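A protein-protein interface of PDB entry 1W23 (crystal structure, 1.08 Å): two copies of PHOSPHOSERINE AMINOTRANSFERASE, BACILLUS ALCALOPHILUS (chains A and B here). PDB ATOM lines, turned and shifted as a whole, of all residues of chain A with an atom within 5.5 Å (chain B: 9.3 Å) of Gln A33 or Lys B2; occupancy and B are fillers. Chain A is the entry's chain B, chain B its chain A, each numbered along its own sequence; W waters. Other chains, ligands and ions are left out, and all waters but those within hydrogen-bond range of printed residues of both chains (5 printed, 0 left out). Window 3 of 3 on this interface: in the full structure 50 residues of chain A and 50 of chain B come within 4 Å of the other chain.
The backbone carbonyl oxygen (O) of Lys B2 is in hydrogen-bond range of the side-chain amide nitrogen (NE2) of Gln A33 (2.6 Å).
SD of Met A34 is in hydrogen-bond range of ND2 of Asn B6 (3.5 Å).
The side-chain amide nitrogen (ND2) of Asn B6 sits at hydrogen-bond distance from the backbone carbonyl oxygen (O) of Glu A38 (3.3 Å).
ND2 of Asn B8 is in hydrogen-bond range of O of Glu A38 (3.1 Å).
N of Leu B14 lies within hydrogen-bond range of OE2 of Glu A38.
The backbone carbonyl oxygen (O) of Phe B5 lies within hydrogen-bond range of the backbone NH (N) of Val B322 (2.9 Å).
The backbone carbonyl oxygen (O) of Leu A27 is in hydrogen-bond range of the backbone NH (N) of Ser A35 (3.5 Å).
OD1 of Asn A28 sits at hydrogen-bond distance from N of Thr A32 (3.3 Å).
The backbone NH (N) of Gln A33 sits at hydrogen-bond distance from the side-chain amide oxygen (OD1) of Asn A28 (2.8 Å).
OG1 of Thr A32 is in hydrogen-bond range of N of Met A34, 3.1 Å away.
N of Ser A35 sits at hydrogen-bond distance from OE1 of Glu A38, at 2.8 Å.
Leu B19 touches Leu A27 (CB to CD2, 3.7 Å).
CG2 of Val B4 touches O of Thr A32, 3.6 Å away.
NE2 of Gln A33 touches CG1 of Val B1, at 3.1 Å.
CG2 of Val B4 touches CD of Gln A33, at 3.6 Å.
ND2 of Asn B8 touches SD of Met A34 (3.9 Å).
CG1 of Val B322 touches CE of Met A34 (3.9 Å).
Ser A35 touches Leu B19 (OG to CD2, 3.9 Å).
CA of Ala B13 touches OE2 of Glu A38, at 3.6 Å.
Glu A38 touches Leu B19 (OE1 to CD1, 3.6 Å).
Printed residues of chain B within 4 Å of Gln A33: Val B1 (3.1 Å), Lys B2 (2.6 Å) and Val B4 (3.6 Å).
Printed residues of chain B within 4 Å of Thr A32: Val B4 (3.6 Å).
Of the printed residues of chain A, Leu B14 touches Glu A38 (2.9 Å).
Of the printed residues of chain A, Val B322 touches Met A34.
Gln B3 touches none of the printed residues of chain A.
Asp A31 touches none of the printed residues of chain B.
The nearest printed residue of chain B that does not touch Gln A33 is Lys B16 (4.6 Å).
The nearest printed residue of chain A that does not touch Lys B2 is Asp A31 (4.4 Å).
Hydrophobic or aromatic side chains of chain B within 4 Å of the printed part of chain A: Val B1, Val B4, Leu B14, Leu B19 and Val B322.
Printed residues of chain A that touch a printed residue of chain B: Leu A27, Thr A32, Gln A33, Met A34, Ser A35 and Glu A38.
Among the printed residues, 14 pairs touch across the chains.
Among the printed residues, no Asp or Glu carboxylate lies within 4 Å of a Lys or Arg side-chain nitrogen of the other chain.
No position is printed for both chains.
Water W5 lies within hydrogen-bond range of O of Gln A33 (2.7 Å), NZ of Lys B16 (2.8 Å) and O of Leu A27 (3.4 Å).
Water W4 bridges the side-chain carboxylate (OE2) of Glu A38 (2.7 Å) and the backbone carbonyl oxygen (O) of Leu B14 (2.8 Å).
Water W2 lies within hydrogen-bond range of the side-chain amino group (NZ) of Lys B16 (2.8 Å), the side-chain carboxylate (OE1) of Glu A38 (2.8 Å) and the backbone carbonyl oxygen (O) of Leu A27 (2.8 Å).
Water W1 lies within hydrogen-bond range of OE2 of Glu A38 (2.8 Å) and ND2 of Asn B6 (3.0 Å).
Water W3 lies within hydrogen-bond range of the backbone NH of Val B4 (2.8 Å), the side-chain amide oxygen of Gln A33 (2.9 Å) and the backbone carbonyl oxygen of Lys B2 (3.3 Å).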
ATOM      1  N   LEU A  27     -12.009 -24.586 -33.419  1.00  0.00           N
ATOM      2  CA  LEU A  27     -12.759 -25.448 -32.519  1.00  0.00           C
ATOM      3  C   LEU A  27     -12.996 -24.824 -31.151  1.00  0.00           C
ATOM      4  O   LEU A  27     -13.869 -25.229 -30.389  1.00  0.00           O
ATOM      5  CB  LEU A  27     -12.047 -26.793 -32.338  1.00  0.00           C
ATOM      6  CG  LEU A  27     -11.524 -27.521 -33.594  1.00  0.00           C
ATOM      7  CD1 LEU A  27     -10.915 -28.850 -33.178  1.00  0.00           C
ATOM      8  CD2 LEU A  27     -12.626 -27.709 -34.604  1.00  0.00           C
ATOM      9  N   ASN A  28     -12.143 -23.855 -30.770  1.00  0.00           N
ATOM     10  CA  ASN A  28     -12.112 -23.282 -29.433  1.00  0.00           C
ATOM     11  C   ASN A  28     -11.782 -21.806 -29.512  1.00  0.00           C
ATOM     12  O   ASN A  28     -10.620 -21.385 -29.466  1.00  0.00           O
ATOM     13  CB  ASN A  28     -11.084 -23.983 -28.551  1.00  0.00           C
ATOM     14  CG  ASN A  28     -11.001 -23.402 -27.172  1.00  0.00           C
ATOM     15  OD1 ASN A  28     -11.847 -22.639 -26.747  1.00  0.00           O
ATOM     16  ND2 ASN A  28      -9.965 -23.784 -26.437  1.00  0.00           N
ATOM     17  N   PHE A  29     -12.834 -21.016 -29.704  1.00  0.00           N
ATOM     18  CA  PHE A  29     -12.719 -19.550 -29.794  1.00  0.00           C
ATOM     19  C   PHE A  29     -12.727 -18.932 -28.412  1.00  0.00           C
ATOM     20  O   PHE A  29     -13.639 -19.164 -27.626  1.00  0.00           O
ATOM     21  CB  PHE A  29     -13.904 -19.013 -30.622  1.00  0.00           C
ATOM     22  CG  PHE A  29     -13.982 -17.496 -30.565  1.00  0.00           C
ATOM     23  CD1 PHE A  29     -13.077 -16.735 -31.302  1.00  0.00           C
ATOM     24  CD2 PHE A  29     -14.915 -16.886 -29.789  1.00  0.00           C
ATOM     25  CE1 PHE A  29     -13.131 -15.351 -31.205  1.00  0.00           C
ATOM     26  CE2 PHE A  29     -14.960 -15.485 -29.703  1.00  0.00           C
ATOM     27  CZ  PHE A  29     -14.074 -14.723 -30.412  1.00  0.00           C
ATOM     28  N   ASP A  31     -11.334 -19.332 -25.566  1.00  0.00           N
ATOM     29  CA  ASP A  31     -11.406 -20.252 -24.443  1.00  0.00           C
ATOM     30  C   ASP A  31     -12.807 -20.681 -24.100  1.00  0.00           C
ATOM     31  O   ASP A  31     -13.095 -21.202 -23.012  1.00  0.00           O
ATOM     32  CB  ASP A  31     -10.701 -19.620 -23.214  1.00  0.00           C
ATOM     33  CG  ASP A  31      -9.196 -19.448 -23.442  1.00  0.00           C
ATOM     34  OD1 ASP A  31      -8.558 -20.459 -23.768  1.00  0.00           O
ATOM     35  OD2 ASP A  31      -8.730 -18.301 -23.278  1.00  0.00           O
ATOM     36  N   THR A  32     -13.759 -20.552 -25.051  1.00  0.00           N
ATOM     37  CA  THR A  32     -15.137 -20.990 -24.793  1.00  0.00           C
ATOM     38  C   THR A  32     -15.383 -22.474 -25.034  1.00  0.00           C
ATOM     39  O   THR A  32     -16.424 -22.995 -24.657  1.00  0.00           O
ATOM     40  CB  THR A  32     -16.136 -20.254 -25.689  1.00  0.00           C
ATOM     41  OG1 THR A  32     -15.951 -20.637 -27.064  1.00  0.00           O
ATOM     42  CG2 THR A  32     -16.068 -18.735 -25.533  1.00  0.00           C
ATOM     43  N   GLN A  33     -14.436 -23.126 -25.679  1.00  0.00           N
ATOM     44  CA  GLN A  33     -14.541 -24.507 -26.117  1.00  0.00           C
ATOM     45  C   GLN A  33     -15.601 -24.696 -27.208  1.00  0.00           C
ATOM     46  O   GLN A  33     -15.972 -25.830 -27.492  1.00  0.00           O
ATOM     47  CB  GLN A  33     -14.740 -25.493 -24.953  1.00  0.00           C
ATOM     48  CG  GLN A  33     -13.616 -25.389 -23.962  1.00  0.00           C
ATOM     49  CD  GLN A  33     -13.700 -26.430 -22.874  1.00  0.00           C
ATOM     50  OE1 GLN A  33     -14.191 -27.534 -23.094  1.00  0.00           O
ATOM     51  NE2 GLN A  33     -13.194 -26.041 -21.711  1.00  0.00           N
ATOM     52  N   MET A  34     -16.009 -23.614 -27.850  1.00  0.00           N
ATOM     53  CA  MET A  34     -16.920 -23.646 -28.991  1.00  0.00           C
ATOM     54  C   MET A  34     -16.234 -22.918 -30.134  1.00  0.00           C
ATOM     55  O   MET A  34     -15.482 -21.961 -29.946  1.00  0.00           O
ATOM     56  CB  MET A  34     -18.223 -22.910 -28.644  1.00  0.00           C
ATOM     57  CG  MET A  34     -19.072 -23.628 -27.595  1.00  0.00           C
ATOM     58  SD  MET A  34     -20.504 -22.698 -27.050  1.00  0.00           S
ATOM     59  CE  MET A  34     -19.719 -21.494 -25.991  1.00  0.00           C
ATOM     60  N   SER A  35     -16.581 -23.292 -31.369  1.00  0.00           N
ATOM     61  CA  SER A  35     -16.216 -22.499 -32.542  1.00  0.00           C
ATOM     62  C   SER A  35     -16.984 -21.193 -32.472  1.00  0.00           C
ATOM     63  O   SER A  35     -18.110 -21.123 -31.954  1.00  0.00           O
ATOM     64  CB  SER A  35     -16.661 -23.254 -33.785  1.00  0.00           C
ATOM     65  OG  SER A  35     -16.295 -22.548 -34.978  1.00  0.00           O
ATOM     66  N   GLU A  38     -20.510 -21.711 -33.467  1.00  0.00           N
ATOM     67  CA  GLU A  38     -21.409 -22.408 -32.556  1.00  0.00           C
ATOM     68  C   GLU A  38     -21.929 -21.492 -31.444  1.00  0.00           C
ATOM     69  O   GLU A  38     -22.678 -21.983 -30.576  1.00  0.00           O
ATOM     70  CB  GLU A  38     -20.664 -23.597 -31.907  1.00  0.00           C
ATOM     71  CG  GLU A  38     -20.273 -24.682 -32.863  1.00  0.00           C
ATOM     72  CD  GLU A  38     -19.494 -25.781 -32.188  1.00  0.00           C
ATOM     73  OE1 GLU A  38     -18.338 -25.496 -31.748  1.00  0.00           O
ATOM     74  OE2 GLU A  38     -20.014 -26.909 -32.085  1.00  0.00           O
ATOM     75  N   VAL B   1      -9.517 -29.553 -19.417  1.00  0.00           N
ATOM     76  CA  VAL B   1     -10.369 -28.467 -19.897  1.00  0.00           C
ATOM     77  C   VAL B   1     -11.640 -28.339 -19.046  1.00  0.00           C
ATOM     78  O   VAL B   1     -12.131 -29.409 -18.657  1.00  0.00           O
ATOM     79  CB  VAL B   1     -10.845 -28.638 -21.354  1.00  0.00           C
ATOM     80  CG1 VAL B   1     -10.479 -27.406 -22.158  1.00  0.00           C
ATOM     81  CG2 VAL B   1     -10.275 -29.891 -21.996  1.00  0.00           C
ATOM     82  N   LYS B   2     -12.077 -27.093 -18.831  1.00  0.00           N
ATOM     83  CA  LYS B   2     -13.348 -26.837 -18.163  1.00  0.00           C
ATOM     84  C   LYS B   2     -14.441 -27.591 -18.924  1.00  0.00           C
ATOM     85  O   LYS B   2     -14.311 -27.783 -20.139  1.00  0.00           O
ATOM     86  CB  LYS B   2     -13.773 -25.374 -18.087  1.00  0.00           C
ATOM     87  CG  LYS B   2     -14.467 -24.761 -19.286  1.00  0.00           C
ATOM     88  CD  LYS B   2     -14.366 -23.261 -19.389  1.00  0.00           C
ATOM     89  CE  LYS B   2     -15.550 -22.479 -18.880  1.00  0.00           C
ATOM     90  NZ  LYS B   2     -16.806 -23.117 -18.348  1.00  0.00           N
ATOM     91  N   GLN B   3     -15.492 -27.985 -18.218  1.00  0.00           N
ATOM     92  CA  GLN B   3     -16.554 -28.692 -18.955  1.00  0.00           C
ATOM     93  C   GLN B   3     -17.436 -27.669 -19.629  1.00  0.00           C
ATOM     94  O   GLN B   3     -17.776 -26.656 -18.993  1.00  0.00           O
ATOM     95  CB  GLN B   3     -17.344 -29.520 -17.947  1.00  0.00           C
ATOM     96  CG  GLN B   3     -18.264 -28.850 -16.941  1.00  0.00           C
ATOM     97  CD  GLN B   3     -18.995 -29.744 -15.961  1.00  0.00           C
ATOM     98  OE1 GLN B   3     -19.854 -29.327 -15.143  1.00  0.00           O
ATOM     99  NE2 GLN B   3     -18.706 -31.071 -15.922  1.00  0.00           N
ATOM    100  N   VAL B   4     -17.821 -27.862 -20.881  1.00  0.00           N
ATOM    101  CA  VAL B   4     -18.751 -26.957 -21.581  1.00  0.00           C
ATOM    102  C   VAL B   4     -19.847 -27.775 -22.245  1.00  0.00           C
ATOM    103  O   VAL B   4     -19.565 -28.721 -22.961  1.00  0.00           O
ATOM    104  CB  VAL B   4     -17.994 -26.114 -22.616  1.00  0.00           C
ATOM    105  CG1 VAL B   4     -18.976 -25.298 -23.429  1.00  0.00           C
ATOM    106  CG2 VAL B   4     -16.998 -25.239 -21.891  1.00  0.00           C
ATOM    107  N   PHE B   5     -21.093 -27.395 -22.016  1.00  0.00           N
ATOM    108  CA  PHE B   5     -22.257 -28.078 -22.607  1.00  0.00           C
ATOM    109  C   PHE B   5     -23.017 -27.034 -23.422  1.00  0.00           C
ATOM    110  O   PHE B   5     -23.562 -26.079 -22.867  1.00  0.00           O
ATOM    111  CB  PHE B   5     -23.140 -28.678 -21.520  1.00  0.00           C
ATOM    112  CG  PHE B   5     -22.369 -29.542 -20.549  1.00  0.00           C
ATOM    113  CD1 PHE B   5     -22.082 -29.100 -19.265  1.00  0.00           C
ATOM    114  CD2 PHE B   5     -21.937 -30.800 -20.943  1.00  0.00           C
ATOM    115  CE1 PHE B   5     -21.387 -29.844 -18.356  1.00  0.00           C
ATOM    116  CE2 PHE B   5     -21.235 -31.580 -20.027  1.00  0.00           C
ATOM    117  CZ  PHE B   5     -20.972 -31.084 -18.764  1.00  0.00           C
ATOM    118  N   ASN B   6     -23.059 -27.206 -24.733  1.00  0.00           N
ATOM    119  CA  ASN B   6     -23.577 -26.182 -25.644  1.00  0.00           C
ATOM    120  C   ASN B   6     -25.044 -26.419 -26.012  1.00  0.00           C
ATOM    121  O   ASN B   6     -25.362 -27.181 -26.934  1.00  0.00           O
ATOM    122  CB  ASN B   6     -22.727 -26.109 -26.896  1.00  0.00           C
ATOM    123  CG  ASN B   6     -23.143 -24.956 -27.805  1.00  0.00           C
ATOM    124  OD1 ASN B   6     -24.074 -24.234 -27.478  1.00  0.00           O
ATOM    125  ND2 ASN B   6     -22.447 -24.843 -28.942  1.00  0.00           N
ATOM    126  N   ASN B   8     -26.965 -23.817 -26.946  1.00  0.00           N
ATOM    127  CA  ASN B   8     -27.353 -22.601 -27.662  1.00  0.00           C
ATOM    128  C   ASN B   8     -28.483 -22.856 -28.656  1.00  0.00           C
ATOM    129  O   ASN B   8     -28.558 -23.900 -29.334  1.00  0.00           O
ATOM    130  CB  ASN B   8     -26.130 -22.033 -28.424  1.00  0.00           C
ATOM    131  CG  ASN B   8     -25.265 -21.166 -27.564  1.00  0.00           C
ATOM    132  OD1 ASN B   8     -25.738 -20.536 -26.614  1.00  0.00           O
ATOM    133  ND2 ASN B   8     -23.983 -21.082 -27.897  1.00  0.00           N
ATOM    134  N   ALA B  13     -24.617 -25.822 -31.589  1.00  0.00           N
ATOM    135  CA  ALA B  13     -23.595 -26.863 -31.695  1.00  0.00           C
ATOM    136  C   ALA B  13     -23.545 -27.434 -33.112  1.00  0.00           C
ATOM    137  O   ALA B  13     -24.588 -27.709 -33.720  1.00  0.00           O
ATOM    138  CB  ALA B  13     -23.924 -28.002 -30.706  1.00  0.00           C
ATOM    139  N   LEU B  14     -22.355 -27.689 -33.598  1.00  0.00           N
ATOM    140  CA  LEU B  14     -22.106 -28.396 -34.862  1.00  0.00           C
ATOM    141  C   LEU B  14     -21.485 -29.750 -34.567  1.00  0.00           C
ATOM    142  O   LEU B  14     -20.886 -29.929 -33.486  1.00  0.00           O
ATOM    143  CB  LEU B  14     -21.267 -27.519 -35.797  1.00  0.00           C
ATOM    144  CG  LEU B  14     -21.960 -26.241 -36.294  1.00  0.00           C
ATOM    145  CD1 LEU B  14     -20.979 -25.277 -36.946  1.00  0.00           C
ATOM    146  CD2 LEU B  14     -23.035 -26.536 -37.323  1.00  0.00           C
ATOM    147  N   LYS B  16     -18.697 -32.193 -34.314  1.00  0.00           N
ATOM    148  CA  LYS B  16     -17.235 -31.964 -34.304  1.00  0.00           C
ATOM    149  C   LYS B  16     -16.549 -32.469 -35.592  1.00  0.00           C
ATOM    150  O   LYS B  16     -15.676 -31.764 -36.061  1.00  0.00           O
ATOM    151  CB  LYS B  16     -16.629 -32.593 -33.070  1.00  0.00           C
ATOM    152  CG  LYS B  16     -15.193 -32.214 -32.843  1.00  0.00           C
ATOM    153  CD  LYS B  16     -15.027 -30.772 -32.404  1.00  0.00           C
ATOM    154  CE  LYS B  16     -15.379 -30.648 -30.928  1.00  0.00           C
ATOM    155  NZ  LYS B  16     -15.040 -29.297 -30.378  1.00  0.00           N
ATOM    156  N   LEU B  19     -16.404 -29.720 -38.217  1.00  0.00           N
ATOM    157  CA  LEU B  19     -15.477 -28.657 -37.840  1.00  0.00           C
ATOM    158  C   LEU B  19     -14.038 -29.120 -37.968  1.00  0.00           C
ATOM    159  O   LEU B  19     -13.182 -28.325 -38.412  1.00  0.00           O
ATOM    160  CB  LEU B  19     -15.769 -28.140 -36.420  1.00  0.00           C
ATOM    161  CG  LEU B  19     -17.015 -27.241 -36.301  1.00  0.00           C
ATOM    162  CD1 LEU B  19     -17.404 -27.137 -34.826  1.00  0.00           C
ATOM    163  CD2 LEU B  19     -16.757 -25.883 -36.888  1.00  0.00           C
ATOM    164  N   ALA B 316     -26.290 -23.336 -13.502  1.00  0.00           N
ATOM    165  CA  ALA B 316     -25.996 -23.970 -14.790  1.00  0.00           C
ATOM    166  C   ALA B 316     -24.812 -23.259 -15.450  1.00  0.00           C
ATOM    167  O   ALA B 316     -23.878 -23.893 -15.944  1.00  0.00           O
ATOM    168  CB  ALA B 316     -27.233 -23.928 -15.667  1.00  0.00           C
ATOM    169  N   LYS B 317     -24.811 -21.935 -15.463  1.00  0.00           N
ATOM    170  CA  LYS B 317     -23.723 -21.203 -16.079  1.00  0.00           C
ATOM    171  C   LYS B 317     -22.401 -21.498 -15.383  1.00  0.00           C
ATOM    172  O   LYS B 317     -21.353 -21.699 -16.047  1.00  0.00           O
ATOM    173  CB  LYS B 317     -24.013 -19.694 -16.097  1.00  0.00           C
ATOM    174  CG  LYS B 317     -23.060 -18.825 -16.891  1.00  0.00           C
ATOM    175  CD  LYS B 317     -23.451 -17.334 -16.885  1.00  0.00           C
ATOM    176  CE  LYS B 317     -22.935 -16.581 -18.093  1.00  0.00           C
ATOM    177  NZ  LYS B 317     -23.398 -15.166 -18.257  1.00  0.00           N
ATOM    178  N   GLU B 318     -22.411 -21.541 -14.031  1.00  0.00           N
ATOM    179  CA  GLU B 318     -21.231 -21.849 -13.235  1.00  0.00           C
ATOM    180  C   GLU B 318     -20.690 -23.215 -13.609  1.00  0.00           C
ATOM    181  O   GLU B 318     -19.460 -23.402 -13.589  1.00  0.00           O
ATOM    182  CB  GLU B 318     -21.600 -21.773 -11.744  1.00  0.00           C
ATOM    183  CG  GLU B 318     -20.471 -22.066 -10.789  1.00  0.00           C
ATOM    184  CD  GLU B 318     -20.494 -23.366 -10.052  1.00  0.00           C
ATOM    185  OE1 GLU B 318     -21.532 -23.947  -9.685  1.00  0.00           O
ATOM    186  OE2 GLU B 318     -19.332 -23.838  -9.809  1.00  0.00           O
ATOM    187  N   GLN B 319     -21.546 -24.186 -13.893  1.00  0.00           N
ATOM    188  CA  GLN B 319     -21.207 -25.542 -14.206  1.00  0.00           C
ATOM    189  C   GLN B 319     -20.872 -25.786 -15.675  1.00  0.00           C
ATOM    190  O   GLN B 319     -20.590 -26.889 -16.049  1.00  0.00           O
ATOM    191  CB  GLN B 319     -22.321 -26.484 -13.725  1.00  0.00           C
ATOM    192  CG  GLN B 319     -22.465 -26.532 -12.227  1.00  0.00           C
ATOM    193  CD  GLN B 319     -21.263 -27.270 -11.606  1.00  0.00           C
ATOM    194  OE1 GLN B 319     -20.964 -28.412 -12.010  1.00  0.00           O
ATOM    195  NE2 GLN B 319     -20.606 -26.621 -10.647  1.00  0.00           N
ATOM    196  N   GLY B 320     -20.840 -24.727 -16.509  1.00  0.00           N
ATOM    197  CA  GLY B 320     -20.386 -24.866 -17.902  1.00  0.00           C
ATOM    198  C   GLY B 320     -21.461 -25.024 -18.901  1.00  0.00           C
ATOM    199  O   GLY B 320     -21.140 -25.167 -20.093  1.00  0.00           O
ATOM    200  N   PHE B 321     -22.737 -24.907 -18.506  1.00  0.00           N
ATOM    201  CA  PHE B 321     -23.844 -24.974 -19.462  1.00  0.00           C
ATOM    202  C   PHE B 321     -24.015 -23.602 -20.154  1.00  0.00           C
ATOM    203  O   PHE B 321     -24.039 -22.557 -19.496  1.00  0.00           O
ATOM    204  CB  PHE B 321     -25.161 -25.338 -18.761  1.00  0.00           C
ATOM    205  CG  PHE B 321     -25.129 -26.739 -18.202  1.00  0.00           C
ATOM    206  CD1 PHE B 321     -24.548 -27.046 -16.997  1.00  0.00           C
ATOM    207  CD2 PHE B 321     -25.702 -27.788 -18.931  1.00  0.00           C
ATOM    208  CE1 PHE B 321     -24.497 -28.339 -16.533  1.00  0.00           C
ATOM    209  CE2 PHE B 321     -25.619 -29.075 -18.486  1.00  0.00           C
ATOM    210  CZ  PHE B 321     -25.015 -29.352 -17.274  1.00  0.00           C
ATOM    211  N   VAL B 322     -24.142 -23.645 -21.473  1.00  0.00           N
ATOM    212  CA  VAL B 322     -24.266 -22.435 -22.308  1.00  0.00           C
ATOM    213  C   VAL B 322     -25.623 -22.440 -22.981  1.00  0.00           C
ATOM    214  O   VAL B 322     -26.029 -23.437 -23.585  1.00  0.00           O
ATOM    215  CB  VAL B 322     -23.126 -22.425 -23.382  1.00  0.00           C
ATOM    216  CG1 VAL B 322     -23.269 -21.241 -24.288  1.00  0.00           C
ATOM    217  CG2 VAL B 322     -21.770 -22.391 -22.690  1.00  0.00           C
HETATM  218  O   HOH W   1     -20.483 -27.049 -29.342  1.00  0.00           O
HETATM  219  O   HOH W   2     -15.908 -26.891 -31.414  1.00  0.00           O
HETATM  220  O   HOH W   3     -16.087 -29.588 -22.302  1.00  0.00           O
HETATM  221  O   HOH W   4     -18.618 -29.263 -31.931  1.00  0.00           O
HETATM  222  O   HOH W   5     -14.198 -27.777 -28.147  1.00  0.00           O
